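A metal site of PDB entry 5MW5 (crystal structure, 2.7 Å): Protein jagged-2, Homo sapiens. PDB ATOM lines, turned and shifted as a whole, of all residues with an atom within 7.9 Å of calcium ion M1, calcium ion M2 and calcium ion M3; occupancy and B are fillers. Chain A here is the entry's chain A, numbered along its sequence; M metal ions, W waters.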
ATOM      1  N   LEU A  18       5.007 -20.748  23.446  1.00  0.00           N
ATOM      2  CA  LEU A  18       6.367 -21.176  23.180  1.00  0.00           C
ATOM      3  C   LEU A  18       7.321 -20.454  24.138  1.00  0.00           C
ATOM      4  O   LEU A  18       6.926 -19.558  24.882  1.00  0.00           O
ATOM      5  CB  LEU A  18       6.765 -20.909  21.723  1.00  0.00           C
ATOM      6  CG  LEU A  18       5.797 -21.353  20.620  1.00  0.00           C
ATOM      7  CD1 LEU A  18       5.330 -20.149  19.834  1.00  0.00           C
ATOM      8  CD2 LEU A  18       6.427 -22.385  19.701  1.00  0.00           C
ATOM      9  N   CYS A  23       2.345 -17.112  20.826  1.00  0.00           N
ATOM     10  CA  CYS A  23       1.452 -18.239  20.677  1.00  0.00           C
ATOM     11  C   CYS A  23       1.951 -19.149  19.562  1.00  0.00           C
ATOM     12  O   CYS A  23       2.564 -18.692  18.586  1.00  0.00           O
ATOM     13  CB  CYS A  23       0.025 -17.768  20.381  1.00  0.00           C
ATOM     14  SG  CYS A  23      -0.740 -16.776  21.690  1.00  0.00           S
ATOM     15  N   CYS A  24       1.677 -20.449  19.707  1.00  0.00           N
ATOM     16  CA  CYS A  24       2.174 -21.428  18.745  1.00  0.00           C
ATOM     17  C   CYS A  24       1.635 -21.152  17.346  1.00  0.00           C
ATOM     18  O   CYS A  24       2.407 -20.930  16.395  1.00  0.00           O
ATOM     19  CB  CYS A  24       1.798 -22.832  19.197  1.00  0.00           C
ATOM     20  SG  CYS A  24       2.812 -23.498  20.528  1.00  0.00           S
ATOM     21  N   ASP A  25       0.324 -21.153  17.194  1.00  0.00           N
ATOM     22  CA  ASP A  25      -0.299 -20.928  15.898  1.00  0.00           C
ATOM     23  C   ASP A  25      -1.353 -19.829  15.972  1.00  0.00           C
ATOM     24  O   ASP A  25      -1.102 -18.694  15.586  1.00  0.00           O
ATOM     25  CB  ASP A  25      -0.908 -22.228  15.375  1.00  0.00           C
ATOM     26  CG  ASP A  25       0.101 -23.353  15.283  1.00  0.00           C
ATOM     27  OD1 ASP A  25       1.306 -23.057  15.141  1.00  0.00           O
ATOM     28  OD2 ASP A  25      -0.302 -24.532  15.349  1.00  0.00           O
ATOM     29  N   HIS A  38      -7.314 -21.107  19.687  1.00  0.00           N
ATOM     30  CA  HIS A  38      -7.735 -22.502  19.585  1.00  0.00           C
ATOM     31  C   HIS A  38      -6.878 -23.358  18.667  1.00  0.00           C
ATOM     32  O   HIS A  38      -6.876 -24.580  18.832  1.00  0.00           O
ATOM     33  CB  HIS A  38      -9.191 -22.590  19.104  1.00  0.00           C
ATOM     34  CG  HIS A  38     -10.201 -22.549  20.219  1.00  0.00           C
ATOM     35  ND1 HIS A  38     -10.208 -23.478  21.237  1.00  0.00           N
ATOM     36  CD2 HIS A  38     -11.214 -21.692  20.466  1.00  0.00           C
ATOM     37  CE1 HIS A  38     -11.197 -23.190  22.069  1.00  0.00           C
ATOM     38  NE2 HIS A  38     -11.818 -22.120  21.622  1.00  0.00           N
ATOM     39  N   ASP A  39      -6.151 -22.770  17.713  1.00  0.00           N
ATOM     40  CA  ASP A  39      -5.184 -23.523  16.915  1.00  0.00           C
ATOM     41  C   ASP A  39      -4.006 -23.886  17.813  1.00  0.00           C
ATOM     42  O   ASP A  39      -3.126 -23.061  18.062  1.00  0.00           O
ATOM     43  CB  ASP A  39      -4.751 -22.716  15.704  1.00  0.00           C
ATOM     44  CG  ASP A  39      -3.929 -23.525  14.713  1.00  0.00           C
ATOM     45  OD1 ASP A  39      -3.714 -24.727  14.951  1.00  0.00           O
ATOM     46  OD2 ASP A  39      -3.517 -22.957  13.679  1.00  0.00           O
ATOM     47  N   GLU A  40      -4.000 -25.121  18.317  1.00  0.00           N
ATOM     48  CA  GLU A  40      -3.096 -25.495  19.394  1.00  0.00           C
ATOM     49  C   GLU A  40      -1.676 -25.706  18.880  1.00  0.00           C
ATOM     50  O   GLU A  40      -1.408 -25.713  17.680  1.00  0.00           O
ATOM     51  CB  GLU A  40      -3.587 -26.764  20.086  1.00  0.00           C
ATOM     52  CG  GLU A  40      -5.036 -26.711  20.530  1.00  0.00           C
ATOM     53  CD  GLU A  40      -5.212 -27.253  21.933  1.00  0.00           C
ATOM     54  OE1 GLU A  40      -6.298 -27.031  22.518  1.00  0.00           O
ATOM     55  OE2 GLU A  40      -4.267 -27.884  22.463  1.00  0.00           O
ATOM     56  N   CYS A  41      -0.770 -25.892  19.835  1.00  0.00           N
ATOM     57  CA  CYS A  41       0.587 -26.315  19.506  1.00  0.00           C
ATOM     58  C   CYS A  41       0.560 -27.747  18.989  1.00  0.00           C
ATOM     59  O   CYS A  41      -0.115 -28.612  19.565  1.00  0.00           O
ATOM     60  CB  CYS A  41       1.493 -26.216  20.738  1.00  0.00           C
ATOM     61  SG  CYS A  41       1.482 -24.624  21.574  1.00  0.00           S
ATOM     62  N   ASP A  42       1.266 -27.997  17.898  1.00  0.00           N
ATOM     63  CA  ASP A  42       1.385 -29.344  17.336  1.00  0.00           C
ATOM     64  C   ASP A  42       2.706 -29.902  17.849  1.00  0.00           C
ATOM     65  O   ASP A  42       3.755 -29.769  17.217  1.00  0.00           O
ATOM     66  CB  ASP A  42       1.298 -29.298  15.819  1.00  0.00           C
ATOM     67  CG  ASP A  42       0.238 -28.307  15.329  1.00  0.00           C
ATOM     68  OD1 ASP A  42      -0.967 -28.546  15.550  1.00  0.00           O
ATOM     69  OD2 ASP A  42       0.623 -27.279  14.728  1.00  0.00           O
ATOM     70  N   THR A  43       2.642 -30.549  19.009  1.00  0.00           N
ATOM     71  CA  THR A  43       3.812 -30.782  19.842  1.00  0.00           C
ATOM     72  C   THR A  43       4.519 -32.090  19.482  1.00  0.00           C
ATOM     73  O   THR A  43       3.883 -33.142  19.390  1.00  0.00           O
ATOM     74  CB  THR A  43       3.407 -30.813  21.316  1.00  0.00           C
ATOM     75  OG1 THR A  43       2.723 -29.591  21.650  1.00  0.00           O
ATOM     76  CG2 THR A  43       4.623 -30.965  22.214  1.00  0.00           C
ATOM     77  N   GLY A  73       0.316 -34.558  20.332  1.00  0.00           N
ATOM     78  CA  GLY A  73      -0.918 -33.967  20.791  1.00  0.00           C
ATOM     79  C   GLY A  73      -0.879 -32.459  20.690  1.00  0.00           C
ATOM     80  O   GLY A  73      -0.023 -31.875  20.027  1.00  0.00           O
ATOM     81  N   GLY A  74      -1.846 -31.832  21.360  1.00  0.00           N
ATOM     82  CA  GLY A  74      -2.006 -30.396  21.304  1.00  0.00           C
ATOM     83  C   GLY A  74      -1.216 -29.647  22.352  1.00  0.00           C
ATOM     84  O   GLY A  74      -0.002 -29.454  22.218  1.00  0.00           O
ATOM     85  N   TRP A 123       8.568 -28.964  20.746  1.00  0.00           N
ATOM     86  CA  TRP A 123       8.497 -28.135  19.553  1.00  0.00           C
ATOM     87  C   TRP A 123       7.089 -28.117  18.995  1.00  0.00           C
ATOM     88  O   TRP A 123       6.377 -29.124  19.044  1.00  0.00           O
ATOM     89  CB  TRP A 123       9.455 -28.630  18.467  1.00  0.00           C
ATOM     90  CG  TRP A 123      10.908 -28.465  18.786  1.00  0.00           C
ATOM     91  CD1 TRP A 123      11.657 -29.256  19.606  1.00  0.00           C
ATOM     92  CD2 TRP A 123      11.792 -27.456  18.282  1.00  0.00           C
ATOM     93  NE1 TRP A 123      12.947 -28.801  19.646  1.00  0.00           N
ATOM     94  CE2 TRP A 123      13.058 -27.688  18.842  1.00  0.00           C
ATOM     95  CE3 TRP A 123      11.627 -26.375  17.418  1.00  0.00           C
ATOM     96  CZ2 TRP A 123      14.155 -26.891  18.566  1.00  0.00           C
ATOM     97  CZ3 TRP A 123      12.725 -25.578  17.142  1.00  0.00           C
ATOM     98  CH2 TRP A 123      13.968 -25.837  17.710  1.00  0.00           C
ATOM     99  N   ASP A 124       6.698 -26.973  18.448  1.00  0.00           N
ATOM    100  CA  ASP A 124       5.498 -26.876  17.615  1.00  0.00           C
ATOM    101  C   ASP A 124       5.892 -27.086  16.161  1.00  0.00           C
ATOM    102  O   ASP A 124       6.804 -26.416  15.653  1.00  0.00           O
ATOM    103  CB  ASP A 124       4.803 -25.520  17.789  1.00  0.00           C
ATOM    104  CG  ASP A 124       3.701 -25.298  16.757  1.00  0.00           C
ATOM    105  OD1 ASP A 124       2.607 -25.874  16.921  1.00  0.00           O
ATOM    106  OD2 ASP A 124       3.922 -24.529  15.799  1.00  0.00           O
ATOM    107  N   TRP A 125       5.220 -28.023  15.502  1.00  0.00           N
ATOM    108  CA  TRP A 125       5.384 -28.248  14.079  1.00  0.00           C
ATOM    109  C   TRP A 125       4.398 -27.364  13.325  1.00  0.00           C
ATOM    110  O   TRP A 125       3.281 -27.112  13.782  1.00  0.00           O
ATOM    111  CB  TRP A 125       5.179 -29.730  13.757  1.00  0.00           C
ATOM    112  CG  TRP A 125       4.987 -30.039  12.312  1.00  0.00           C
ATOM    113  CD1 TRP A 125       5.943 -30.423  11.425  1.00  0.00           C
ATOM    114  CD2 TRP A 125       3.753 -30.008  11.591  1.00  0.00           C
ATOM    115  NE1 TRP A 125       5.384 -30.631  10.184  1.00  0.00           N
ATOM    116  CE2 TRP A 125       4.036 -30.382  10.268  1.00  0.00           C
ATOM    117  CE3 TRP A 125       2.440 -29.692  11.936  1.00  0.00           C
ATOM    118  CZ2 TRP A 125       3.051 -30.446   9.291  1.00  0.00           C
ATOM    119  CZ3 TRP A 125       1.465 -29.757  10.972  1.00  0.00           C
ATOM    120  CH2 TRP A 125       1.775 -30.128   9.658  1.00  0.00           C
ATOM    121  N   ASP A 126       4.819 -26.881  12.144  1.00  0.00           N
ATOM    122  CA  ASP A 126       4.113 -25.790  11.499  1.00  0.00           C
ATOM    123  C   ASP A 126       3.823 -25.952  10.011  1.00  0.00           C
ATOM    124  O   ASP A 126       3.334 -25.006   9.387  1.00  0.00           O
ATOM    125  CB  ASP A 126       4.894 -24.477  11.687  1.00  0.00           C
ATOM    126  CG  ASP A 126       4.295 -23.588  12.748  1.00  0.00           C
ATOM    127  OD1 ASP A 126       3.427 -24.082  13.495  1.00  0.00           O
ATOM    128  OD2 ASP A 126       4.675 -22.408  12.836  1.00  0.00           O
ATOM    129  N   ASN A 127       4.101 -27.129   9.430  1.00  0.00           N
ATOM    130  CA  ASN A 127       3.907 -27.360   7.993  1.00  0.00           C
ATOM    131  C   ASN A 127       4.699 -26.334   7.170  1.00  0.00           C
ATOM    132  O   ASN A 127       4.148 -25.455   6.501  1.00  0.00           O
ATOM    133  CB  ASN A 127       2.421 -27.344   7.627  1.00  0.00           C
ATOM    134  CG  ASN A 127       2.172 -27.567   6.146  1.00  0.00           C
ATOM    135  OD1 ASN A 127       2.989 -28.161   5.445  1.00  0.00           O
ATOM    136  ND2 ASN A 127       1.032 -27.086   5.652  1.00  0.00           N
ATOM    137  N   ASN A 132      12.735 -23.437  11.184  1.00  0.00           N
ATOM    138  CA  ASN A 132      12.464 -22.260  12.014  1.00  0.00           C
ATOM    139  C   ASN A 132      12.721 -22.632  13.472  1.00  0.00           C
ATOM    140  O   ASN A 132      11.938 -23.355  14.087  1.00  0.00           O
ATOM    141  CB  ASN A 132      11.028 -21.793  11.799  1.00  0.00           C
ATOM    142  CG  ASN A 132      10.684 -20.550  12.604  1.00  0.00           C
ATOM    143  OD1 ASN A 132      11.542 -19.945  13.250  1.00  0.00           O
ATOM    144  ND2 ASN A 132       9.409 -20.168  12.572  1.00  0.00           N
ATOM    145  N   GLU A 134      12.664 -20.683  16.064  1.00  0.00           N
ATOM    146  CA  GLU A 134      11.843 -19.896  16.985  1.00  0.00           C
ATOM    147  C   GLU A 134      10.640 -20.694  17.489  1.00  0.00           C
ATOM    148  O   GLU A 134       9.955 -20.268  18.428  1.00  0.00           O
ATOM    149  CB  GLU A 134      11.388 -18.601  16.300  1.00  0.00           C
ATOM    150  CG  GLU A 134      10.744 -17.584  17.243  1.00  0.00           C
ATOM    151  CD  GLU A 134      10.888 -16.154  16.766  1.00  0.00           C
ATOM    152  OE1 GLU A 134      11.294 -15.301  17.577  1.00  0.00           O
ATOM    153  OE2 GLU A 134      10.573 -15.881  15.588  1.00  0.00           O
ATOM    154  N   LEU A 135      10.376 -21.853  16.882  1.00  0.00           N
ATOM    155  CA  LEU A 135       9.244 -22.688  17.236  1.00  0.00           C
ATOM    156  C   LEU A 135       9.532 -23.616  18.408  1.00  0.00           C
ATOM    157  O   LEU A 135       8.915 -24.692  18.507  1.00  0.00           O
ATOM    158  CB  LEU A 135       8.807 -23.503  16.020  1.00  0.00           C
ATOM    159  CG  LEU A 135       8.230 -22.703  14.843  1.00  0.00           C
ATOM    160  CD1 LEU A 135       7.980 -23.617  13.652  1.00  0.00           C
ATOM    161  CD2 LEU A 135       6.952 -22.008  15.264  1.00  0.00           C
HETATM  162 CA    CA M   1      -1.918 -26.292  15.406  1.00  0.00          CA
HETATM  163 CA    CA M   2       1.893 -25.303  14.761  1.00  0.00          CA
HETATM  164 CA    CA M   3       3.527 -22.296  14.914  1.00  0.00          CA
HETATM  165  O   HOH W   1      -3.846 -27.615  16.090  1.00  0.00           O
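SG of Cys 41 forms a disulfide with SG of Cys 24 (2.0 Å). N of Asp 124 sits at hydrogen-bond distance from O of Leu 135.
The nearest printed residue that does not touch calcium ion M1 is Cys 41 (4.6 Å).
Along chain A the residues within 4 Å of calcium ion M2 span positions 25 to 126.
CD2 of Leu 135 touches calcium ion M3 (3.5 Å). Within 4 Å of calcium ion M3: Cys 24, Asp 25, Asp 124, Asp 126 and Leu 135. Along chain A the residues within 4 Å of calcium ion M3 span positions 24 to 135.
Calcium ion M1 is bound by the side-chain carboxylate (OD2) of Asp 25 (2.4 Å), the backbone carbonyl oxygen (O) of Glu 40 (2.4 Å), the side-chain carboxylate (OD1) of Asp 39 (2.4 Å), water W1 (2.4 Å), the side-chain carboxylate (OD1) of Asp 42 (2.5 Å) and the side-chain carboxylate (OD2) of Asp 42 (2.8 Å). Calcium ion M1 has six donor atoms within binding distance.
Calcium ion M2 is bound by OD1 of Asp 126 (2.3 Å), OD1 of Asp 124 (2.3 Å), OD2 of Asp 42 (2.3 Å), OD1 of Asp 25 (2.4 Å), OD2 of Asp 25 (2.4 Å), OD2 of Asp 124 (2.4 Å) and O of Trp 125 (2.5 Å).
Calcium ion M3 is bound by the side-chain carboxylate (OD1) of Asp 126 (2.3 Å), the backbone carbonyl oxygen (O) of Cys 24 (2.3 Å), the side-chain carboxylate (OD1) of Asp 25 (2.4 Å), the side-chain carboxylate (OD2) of Asp 126 (2.4 Å) and the side-chain carboxylate (OD2) of Asp 124 (2.4 Å). Calcium ion M3 has five donor atoms within binding distance.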
